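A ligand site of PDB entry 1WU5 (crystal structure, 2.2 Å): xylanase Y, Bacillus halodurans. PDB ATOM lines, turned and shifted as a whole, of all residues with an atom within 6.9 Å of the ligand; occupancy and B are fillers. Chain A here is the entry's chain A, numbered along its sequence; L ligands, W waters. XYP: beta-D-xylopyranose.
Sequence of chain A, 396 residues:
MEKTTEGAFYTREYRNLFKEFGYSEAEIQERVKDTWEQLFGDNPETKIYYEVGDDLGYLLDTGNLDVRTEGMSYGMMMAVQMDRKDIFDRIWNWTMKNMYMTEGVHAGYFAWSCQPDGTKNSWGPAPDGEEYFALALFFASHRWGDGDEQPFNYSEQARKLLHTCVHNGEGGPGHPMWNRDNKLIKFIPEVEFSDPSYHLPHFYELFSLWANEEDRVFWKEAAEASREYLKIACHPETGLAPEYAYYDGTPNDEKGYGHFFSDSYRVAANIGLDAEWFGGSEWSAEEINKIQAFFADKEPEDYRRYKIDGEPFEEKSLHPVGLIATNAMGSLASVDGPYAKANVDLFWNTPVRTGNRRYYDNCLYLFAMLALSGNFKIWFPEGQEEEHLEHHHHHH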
ATOM      1  N   ASP A  61      -5.224 -30.512 -27.977  1.00  0.00           N
ATOM      2  CA  ASP A  61      -5.390 -29.504 -26.945  1.00  0.00           C
ATOM      3  C   ASP A  61      -4.988 -30.331 -25.721  1.00  0.00           C
ATOM      4  O   ASP A  61      -5.799 -31.060 -25.154  1.00  0.00           O
ATOM      5  CB  ASP A  61      -6.850 -29.062 -26.797  1.00  0.00           C
ATOM      6  CG  ASP A  61      -7.040 -28.001 -25.715  1.00  0.00           C
ATOM      7  OD1 ASP A  61      -6.370 -28.096 -24.659  1.00  0.00           O
ATOM      8  OD2 ASP A  61      -7.850 -27.074 -25.907  1.00  0.00           O
ATOM      9  N   THR A  62      -3.717 -30.233 -25.360  1.00  0.00           N
ATOM     10  CA  THR A  62      -3.172 -30.981 -24.236  1.00  0.00           C
ATOM     11  C   THR A  62      -3.950 -30.812 -22.933  1.00  0.00           C
ATOM     12  O   THR A  62      -4.058 -31.750 -22.148  1.00  0.00           O
ATOM     13  CB  THR A  62      -1.689 -30.598 -24.005  1.00  0.00           C
ATOM     14  OG1 THR A  62      -1.574 -29.176 -23.872  1.00  0.00           O
ATOM     15  CG2 THR A  62      -0.844 -31.046 -25.184  1.00  0.00           C
ATOM     16  N   GLY A  63      -4.496 -29.614 -22.724  1.00  0.00           N
ATOM     17  CA  GLY A  63      -5.230 -29.341 -21.495  1.00  0.00           C
ATOM     18  C   GLY A  63      -6.635 -29.895 -21.386  1.00  0.00           C
ATOM     19  O   GLY A  63      -7.128 -30.140 -20.277  1.00  0.00           O
ATOM     20  N   ASN A  64      -7.306 -30.103 -22.521  1.00  0.00           N
ATOM     21  CA  ASN A  64      -8.672 -30.623 -22.507  1.00  0.00           C
ATOM     22  C   ASN A  64      -8.775 -31.986 -23.185  1.00  0.00           C
ATOM     23  O   ASN A  64      -9.868 -32.499 -23.396  1.00  0.00           O
ATOM     24  CB  ASN A  64      -9.600 -29.629 -23.189  1.00  0.00           C
ATOM     25  CG  ASN A  64      -9.713 -28.313 -22.436  1.00  0.00           C
ATOM     26  OD1 ASN A  64     -10.272 -28.263 -21.336  1.00  0.00           O
ATOM     27  ND2 ASN A  64      -9.186 -27.249 -23.009  1.00  0.00           N
ATOM     28  N   ASP A  66      -8.580 -33.050 -26.225  1.00  0.00           N
ATOM     29  CA  ASP A  66      -9.477 -33.116 -27.364  1.00  0.00           C
ATOM     30  C   ASP A  66      -8.840 -32.412 -28.563  1.00  0.00           C
ATOM     31  O   ASP A  66      -7.792 -31.769 -28.421  1.00  0.00           O
ATOM     32  CB  ASP A  66     -10.820 -32.464 -27.030  1.00  0.00           C
ATOM     33  CG  ASP A  66     -10.727 -30.968 -26.827  1.00  0.00           C
ATOM     34  OD1 ASP A  66      -9.608 -30.424 -26.808  1.00  0.00           O
ATOM     35  OD2 ASP A  66     -11.790 -30.317 -26.687  1.00  0.00           O
ATOM     36  N   ARG A  68      -9.451 -29.653 -31.485  1.00  0.00           N
ATOM     37  CA  ARG A  68     -10.304 -28.508 -31.792  1.00  0.00           C
ATOM     38  C   ARG A  68     -10.019 -27.912 -33.151  1.00  0.00           C
ATOM     39  O   ARG A  68      -8.855 -27.857 -33.578  1.00  0.00           O
ATOM     40  CB  ARG A  68     -10.125 -27.455 -30.701  1.00  0.00           C
ATOM     41  CG  ARG A  68     -10.255 -28.038 -29.319  1.00  0.00           C
ATOM     42  CD  ARG A  68     -10.112 -27.023 -28.206  1.00  0.00           C
ATOM     43  NE  ARG A  68     -10.663 -27.600 -26.978  1.00  0.00           N
ATOM     44  CZ  ARG A  68     -11.065 -26.899 -25.930  1.00  0.00           C
ATOM     45  NH1 ARG A  68     -10.992 -25.571 -25.934  1.00  0.00           N
ATOM     46  NH2 ARG A  68     -11.593 -27.525 -24.891  1.00  0.00           N
ATOM     47  N   GLU A  70      -9.897 -25.087 -33.815  1.00  0.00           N
ATOM     48  CA  GLU A  70      -8.993 -23.972 -33.563  1.00  0.00           C
ATOM     49  C   GLU A  70      -7.568 -24.486 -33.819  1.00  0.00           C
ATOM     50  O   GLU A  70      -6.791 -23.872 -34.564  1.00  0.00           O
ATOM     51  CB  GLU A  70      -9.114 -23.501 -32.123  1.00  0.00           C
ATOM     52  CG  GLU A  70      -8.057 -22.498 -31.683  1.00  0.00           C
ATOM     53  CD  GLU A  70      -7.988 -22.345 -30.180  1.00  0.00           C
ATOM     54  OE1 GLU A  70      -7.726 -23.365 -29.491  1.00  0.00           O
ATOM     55  OE2 GLU A  70      -8.200 -21.224 -29.683  1.00  0.00           O
ATOM     56  N   GLY A  71      -7.245 -25.611 -33.189  1.00  0.00           N
ATOM     57  CA  GLY A  71      -5.914 -26.186 -33.341  1.00  0.00           C
ATOM     58  C   GLY A  71      -5.636 -26.714 -34.748  1.00  0.00           C
ATOM     59  O   GLY A  71      -4.553 -26.489 -35.290  1.00  0.00           O
ATOM     60  N   TYR A  74      -5.157 -23.877 -37.045  1.00  0.00           N
ATOM     61  CA  TYR A  74      -3.874 -23.270 -36.705  1.00  0.00           C
ATOM     62  C   TYR A  74      -2.768 -24.112 -37.350  1.00  0.00           C
ATOM     63  O   TYR A  74      -1.861 -23.581 -37.987  1.00  0.00           O
ATOM     64  CB  TYR A  74      -3.659 -23.255 -35.197  1.00  0.00           C
ATOM     65  CG  TYR A  74      -4.312 -22.111 -34.443  1.00  0.00           C
ATOM     66  CD1 TYR A  74      -4.949 -21.071 -35.115  1.00  0.00           C
ATOM     67  CD2 TYR A  74      -4.259 -22.072 -33.048  1.00  0.00           C
ATOM     68  CE1 TYR A  74      -5.535 -20.013 -34.414  1.00  0.00           C
ATOM     69  CE2 TYR A  74      -4.840 -21.024 -32.338  1.00  0.00           C
ATOM     70  CZ  TYR A  74      -5.473 -19.995 -33.023  1.00  0.00           C
ATOM     71  OH  TYR A  74      -6.061 -18.977 -32.320  1.00  0.00           O
ATOM     72  N   TRP A 112     -16.529 -28.270 -33.496  1.00  0.00           N
ATOM     73  CA  TRP A 112     -15.421 -27.601 -32.816  1.00  0.00           C
ATOM     74  C   TRP A 112     -14.519 -28.457 -31.943  1.00  0.00           C
ATOM     75  O   TRP A 112     -13.355 -28.108 -31.729  1.00  0.00           O
ATOM     76  CB  TRP A 112     -15.931 -26.422 -31.985  1.00  0.00           C
ATOM     77  CG  TRP A 112     -16.441 -26.786 -30.619  1.00  0.00           C
ATOM     78  CD1 TRP A 112     -17.689 -27.251 -30.302  1.00  0.00           C
ATOM     79  CD2 TRP A 112     -15.711 -26.708 -29.390  1.00  0.00           C
ATOM     80  NE1 TRP A 112     -17.782 -27.456 -28.945  1.00  0.00           N
ATOM     81  CE2 TRP A 112     -16.585 -27.136 -28.364  1.00  0.00           C
ATOM     82  CE3 TRP A 112     -14.408 -26.321 -29.049  1.00  0.00           C
ATOM     83  CZ2 TRP A 112     -16.197 -27.176 -27.008  1.00  0.00           C
ATOM     84  CZ3 TRP A 112     -14.017 -26.362 -27.707  1.00  0.00           C
ATOM     85  CH2 TRP A 112     -14.920 -26.790 -26.710  1.00  0.00           C
ATOM     86  N   ASP A 128     -13.851 -19.051 -35.422  1.00  0.00           N
ATOM     87  CA  ASP A 128     -12.455 -18.699 -35.618  1.00  0.00           C
ATOM     88  C   ASP A 128     -11.704 -19.836 -36.327  1.00  0.00           C
ATOM     89  O   ASP A 128     -10.699 -19.612 -36.998  1.00  0.00           O
ATOM     90  CB  ASP A 128     -11.797 -18.293 -34.277  1.00  0.00           C
ATOM     91  CG  ASP A 128     -11.752 -19.419 -33.256  1.00  0.00           C
ATOM     92  OD1 ASP A 128     -12.706 -20.229 -33.163  1.00  0.00           O
ATOM     93  OD2 ASP A 128     -10.759 -19.483 -32.502  1.00  0.00           O
ATOM     94  N   TYR A 198     -11.708 -13.067 -32.394  1.00  0.00           N
ATOM     95  CA  TYR A 198     -12.142 -13.702 -33.648  1.00  0.00           C
ATOM     96  C   TYR A 198     -12.030 -12.781 -34.868  1.00  0.00           C
ATOM     97  O   TYR A 198     -11.975 -13.257 -36.012  1.00  0.00           O
ATOM     98  CB  TYR A 198     -13.599 -14.154 -33.520  1.00  0.00           C
ATOM     99  CG  TYR A 198     -13.851 -15.393 -32.704  1.00  0.00           C
ATOM    100  CD1 TYR A 198     -12.941 -15.825 -31.734  1.00  0.00           C
ATOM    101  CD2 TYR A 198     -15.028 -16.120 -32.873  1.00  0.00           C
ATOM    102  CE1 TYR A 198     -13.211 -16.944 -30.942  1.00  0.00           C
ATOM    103  CE2 TYR A 198     -15.303 -17.239 -32.091  1.00  0.00           C
ATOM    104  CZ  TYR A 198     -14.398 -17.651 -31.130  1.00  0.00           C
ATOM    105  OH  TYR A 198     -14.686 -18.750 -30.351  1.00  0.00           O
ATOM    106  N   GLU A 243     -13.065 -11.429 -23.582  1.00  0.00           N
ATOM    107  CA  GLU A 243     -13.099 -12.629 -24.398  1.00  0.00           C
ATOM    108  C   GLU A 243     -14.347 -12.608 -25.277  1.00  0.00           C
ATOM    109  O   GLU A 243     -14.260 -12.788 -26.500  1.00  0.00           O
ATOM    110  CB  GLU A 243     -13.076 -13.871 -23.515  1.00  0.00           C
ATOM    111  CG  GLU A 243     -11.803 -14.006 -22.697  1.00  0.00           C
ATOM    112  CD  GLU A 243     -11.711 -15.348 -21.996  1.00  0.00           C
ATOM    113  OE1 GLU A 243     -12.466 -15.574 -21.032  1.00  0.00           O
ATOM    114  OE2 GLU A 243     -10.892 -16.177 -22.420  1.00  0.00           O
ATOM    115  N   PHE A 261      -8.671 -12.512 -20.736  1.00  0.00           N
ATOM    116  CA  PHE A 261      -8.146 -13.841 -20.463  1.00  0.00           C
ATOM    117  C   PHE A 261      -7.753 -14.541 -21.776  1.00  0.00           C
ATOM    118  O   PHE A 261      -7.715 -13.901 -22.832  1.00  0.00           O
ATOM    119  CB  PHE A 261      -9.189 -14.661 -19.707  1.00  0.00           C
ATOM    120  CG  PHE A 261      -8.608 -15.731 -18.814  1.00  0.00           C
ATOM    121  CD1 PHE A 261      -9.039 -17.045 -18.919  1.00  0.00           C
ATOM    122  CD2 PHE A 261      -7.637 -15.415 -17.873  1.00  0.00           C
ATOM    123  CE1 PHE A 261      -8.518 -18.043 -18.095  1.00  0.00           C
ATOM    124  CE2 PHE A 261      -7.102 -16.404 -17.046  1.00  0.00           C
ATOM    125  CZ  PHE A 261      -7.546 -17.718 -17.154  1.00  0.00           C
ATOM    126  N   SER A 262      -7.485 -15.845 -21.697  1.00  0.00           N
ATOM    127  CA  SER A 262      -7.067 -16.651 -22.860  1.00  0.00           C
ATOM    128  C   SER A 262      -7.444 -16.173 -24.272  1.00  0.00           C
ATOM    129  O   SER A 262      -6.555 -15.928 -25.095  1.00  0.00           O
ATOM    130  CB  SER A 262      -7.553 -18.092 -22.673  1.00  0.00           C
ATOM    131  OG  SER A 262      -7.131 -18.588 -21.417  1.00  0.00           O
ATOM    132  N   ASP A 263      -8.733 -16.057 -24.553  1.00  0.00           N
ATOM    133  CA  ASP A 263      -9.154 -15.603 -25.880  1.00  0.00           C
ATOM    134  C   ASP A 263      -8.566 -14.254 -26.234  1.00  0.00           C
ATOM    135  O   ASP A 263      -7.937 -14.084 -27.284  1.00  0.00           O
ATOM    136  CB  ASP A 263     -10.692 -15.506 -25.952  1.00  0.00           C
ATOM    137  CG  ASP A 263     -11.358 -16.837 -26.288  1.00  0.00           C
ATOM    138  OD1 ASP A 263     -10.824 -17.903 -25.916  1.00  0.00           O
ATOM    139  OD2 ASP A 263     -12.433 -16.805 -26.922  1.00  0.00           O
ATOM    140  N   ARG A 266      -5.106 -12.942 -28.206  1.00  0.00           N
ATOM    141  CA  ARG A 266      -4.949 -12.913 -29.648  1.00  0.00           C
ATOM    142  C   ARG A 266      -5.246 -11.580 -30.318  1.00  0.00           C
ATOM    143  O   ARG A 266      -4.841 -11.352 -31.455  1.00  0.00           O
ATOM    144  CB  ARG A 266      -5.812 -14.024 -30.276  1.00  0.00           C
ATOM    145  CG  ARG A 266      -5.339 -15.417 -29.888  1.00  0.00           C
ATOM    146  CD  ARG A 266      -6.303 -16.506 -30.337  1.00  0.00           C
ATOM    147  NE  ARG A 266      -7.633 -16.326 -29.751  1.00  0.00           N
ATOM    148  CZ  ARG A 266      -8.548 -17.286 -29.634  1.00  0.00           C
ATOM    149  NH1 ARG A 266      -8.277 -18.518 -30.061  1.00  0.00           N
ATOM    150  NH2 ARG A 266      -9.730 -17.015 -29.104  1.00  0.00           N
ATOM    151  N   LEU A 318      -3.846 -18.543 -17.235  1.00  0.00           N
ATOM    152  CA  LEU A 318      -3.672 -19.965 -17.509  1.00  0.00           C
ATOM    153  C   LEU A 318      -2.638 -20.189 -18.617  1.00  0.00           C
ATOM    154  O   LEU A 318      -2.026 -21.256 -18.714  1.00  0.00           O
ATOM    155  CB  LEU A 318      -5.011 -20.582 -17.920  1.00  0.00           C
ATOM    156  CG  LEU A 318      -5.037 -22.093 -18.164  1.00  0.00           C
ATOM    157  CD1 LEU A 318      -4.696 -22.824 -16.858  1.00  0.00           C
ATOM    158  CD2 LEU A 318      -6.418 -22.511 -18.668  1.00  0.00           C
ATOM    159  N   HIS A 319      -2.421 -19.169 -19.445  1.00  0.00           N
ATOM    160  CA  HIS A 319      -1.465 -19.259 -20.541  1.00  0.00           C
ATOM    161  C   HIS A 319      -0.615 -17.992 -20.609  1.00  0.00           C
ATOM    162  O   HIS A 319      -0.730 -17.200 -21.551  1.00  0.00           O
ATOM    163  CB  HIS A 319      -2.212 -19.440 -21.865  1.00  0.00           C
ATOM    164  CG  HIS A 319      -3.119 -20.636 -21.880  1.00  0.00           C
ATOM    165  ND1 HIS A 319      -2.642 -21.925 -21.941  1.00  0.00           N
ATOM    166  CD2 HIS A 319      -4.463 -20.735 -21.822  1.00  0.00           C
ATOM    167  CE1 HIS A 319      -3.658 -22.774 -21.926  1.00  0.00           C
ATOM    168  NE2 HIS A 319      -4.777 -22.072 -21.847  1.00  0.00           N
ATOM    169  N   ARG A 357      -0.695 -27.778 -20.341  1.00  0.00           N
ATOM    170  CA  ARG A 357      -1.361 -26.557 -20.774  1.00  0.00           C
ATOM    171  C   ARG A 357      -0.581 -25.857 -21.873  1.00  0.00           C
ATOM    172  O   ARG A 357      -0.881 -24.712 -22.235  1.00  0.00           O
ATOM    173  CB  ARG A 357      -1.535 -25.603 -19.596  1.00  0.00           C
ATOM    174  CG  ARG A 357      -2.545 -26.074 -18.558  1.00  0.00           C
ATOM    175  CD  ARG A 357      -3.921 -26.156 -19.172  1.00  0.00           C
ATOM    176  NE  ARG A 357      -4.939 -26.569 -18.211  1.00  0.00           N
ATOM    177  CZ  ARG A 357      -6.237 -26.632 -18.486  1.00  0.00           C
ATOM    178  NH1 ARG A 357      -6.678 -26.304 -19.694  1.00  0.00           N
ATOM    179  NH2 ARG A 357      -7.093 -27.014 -17.553  1.00  0.00           N
ATOM    180  N   TYR A 359      -0.359 -26.512 -25.188  1.00  0.00           N
ATOM    181  CA  TYR A 359      -1.044 -26.343 -26.470  1.00  0.00           C
ATOM    182  C   TYR A 359      -1.329 -24.902 -26.902  1.00  0.00           C
ATOM    183  O   TYR A 359      -0.779 -24.436 -27.906  1.00  0.00           O
ATOM    184  CB  TYR A 359      -2.346 -27.148 -26.469  1.00  0.00           C
ATOM    185  CG  TYR A 359      -3.335 -26.716 -27.532  1.00  0.00           C
ATOM    186  CD1 TYR A 359      -3.121 -27.027 -28.878  1.00  0.00           C
ATOM    187  CD2 TYR A 359      -4.472 -25.973 -27.196  1.00  0.00           C
ATOM    188  CE1 TYR A 359      -4.028 -26.596 -29.862  1.00  0.00           C
ATOM    189  CE2 TYR A 359      -5.368 -25.542 -28.163  1.00  0.00           C
ATOM    190  CZ  TYR A 359      -5.144 -25.863 -29.491  1.00  0.00           C
ATOM    191  OH  TYR A 359      -6.044 -25.441 -30.444  1.00  0.00           O
ATOM    192  N   TYR A 360      -2.182 -24.209 -26.152  1.00  0.00           N
ATOM    193  CA  TYR A 360      -2.549 -22.840 -26.499  1.00  0.00           C
ATOM    194  C   TYR A 360      -1.360 -21.891 -26.549  1.00  0.00           C
ATOM    195  O   TYR A 360      -1.219 -21.102 -27.493  1.00  0.00           O
ATOM    196  CB  TYR A 360      -3.599 -22.309 -25.512  1.00  0.00           C
ATOM    197  CG  TYR A 360      -4.274 -21.018 -25.951  1.00  0.00           C
ATOM    198  CD1 TYR A 360      -5.028 -20.962 -27.120  1.00  0.00           C
ATOM    199  CD2 TYR A 360      -4.139 -19.844 -25.197  1.00  0.00           C
ATOM    200  CE1 TYR A 360      -5.649 -19.783 -27.533  1.00  0.00           C
ATOM    201  CE2 TYR A 360      -4.764 -18.665 -25.596  1.00  0.00           C
ATOM    202  CZ  TYR A 360      -5.510 -18.639 -26.769  1.00  0.00           C
ATOM    203  OH  TYR A 360      -6.125 -17.469 -27.151  1.00  0.00           O
HETATM  204  O1  XYP L   1      -7.027 -23.174 -22.520  1.00  0.00           O
HETATM  205  C1  XYP L   1      -7.207 -22.619 -23.771  1.00  0.00           C
HETATM  206  C2  XYP L   1      -7.843 -23.643 -24.712  1.00  0.00           C
HETATM  207  C3  XYP L   1      -8.139 -22.987 -26.070  1.00  0.00           C
HETATM  208  C4  XYP L   1      -8.953 -21.696 -25.886  1.00  0.00           C
HETATM  209  C5  XYP L   1      -8.263 -20.772 -24.883  1.00  0.00           C
HETATM  210  O2  XYP L   1      -6.956 -24.738 -24.895  1.00  0.00           O
HETATM  211  O3  XYP L   1      -8.867 -23.892 -26.886  1.00  0.00           O
HETATM  212  O4  XYP L   1      -9.100 -21.033 -27.135  1.00  0.00           O
HETATM  213  O5  XYP L   1      -8.059 -21.468 -23.634  1.00  0.00           O
HETATM  214  O   HOH W   1      -9.241 -24.722 -21.421  1.00  0.00           O
HETATM  215  O   HOH W   2     -11.076 -19.772 -29.381  1.00  0.00           O
HETATM  216  O   HOH W   3      -5.745 -25.793 -22.735  1.00  0.00           O
HETATM  217  O   HOH W   4      -8.879 -20.326 -20.976  1.00  0.00           O
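Merely in contact with the ligand: Asn 64 (3.9 Å), Ser 262 (3.5 Å), Asp 263 (3.8 Å), Arg 266 (3.9 Å), Leu 318 (3.96 Å), Tyr 359 (3.6 Å) and Tyr 360 (3.7 Å).
O of Ser 262 lies within hydrogen-bond range of OH of Tyr 360, at 2.6 Å. The side-chain carboxylate (OD1) of Asp 61 lies within hydrogen-bond range of the backbone NH (N) of Asn 64. The backbone NH of Asp 263 lies within hydrogen-bond range of the side-chain carboxylate of Glu 243, 3.0 Å away. The side-chain carboxylate of Asp 66 is in salt-bridge range of the guanidinium group of Arg 68. OH of Tyr 359 lies within hydrogen-bond range of OE1 of Glu 70, 2.8 Å away. The side-chain hydroxyl of Tyr 360 sits at hydrogen-bond distance from the guanidinium group of Arg 266, 3.2 Å away. N of Gly 71 lies close to OH of Tyr 359. OD2 of Asp 61 lies within salt-bridge range of NE of Arg 68 (3.1 Å).
O4 of the ligand is in hydrogen-bond range of OE2 of Glu 70, 2.7 Å away. The side-chain carboxylate of Asp 61 lies within hydrogen-bond range of an oxygen (O2) of the ligand. The guanidinium group (NH1) of Arg 68 is in hydrogen-bond range of an oxygen (O3) of the ligand (2.9 Å). An oxygen (O1) of the ligand lies within hydrogen-bond range of a ring nitrogen (NE2) of His 319 (2.6 Å).
Water W3 lies within hydrogen-bond range of an oxygen (O2) of the ligand, the side-chain carboxylate (OD1) of Asp 61 and the guanidinium group (NH1) of Arg 357. Water W1 lies within hydrogen-bond range of an oxygen (O1) of the ligand (2.9 Å), the side-chain amide nitrogen of Asn 64 (3.0 Å) and the guanidinium group of Arg 357 (3.5 Å). Water W4 lies within hydrogen-bond range of the side-chain hydroxyl of Ser 262 and an oxygen (O5) of the ligand. Water W2 lies within hydrogen-bond range of the guanidinium group of Arg 266 (3.1 Å), the side-chain carboxylate of Asp 128 (3.2 Å), the side-chain carboxylate of Glu 70 (3.2 Å) and an oxygen (O4) of the ligand (3.2 Å).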
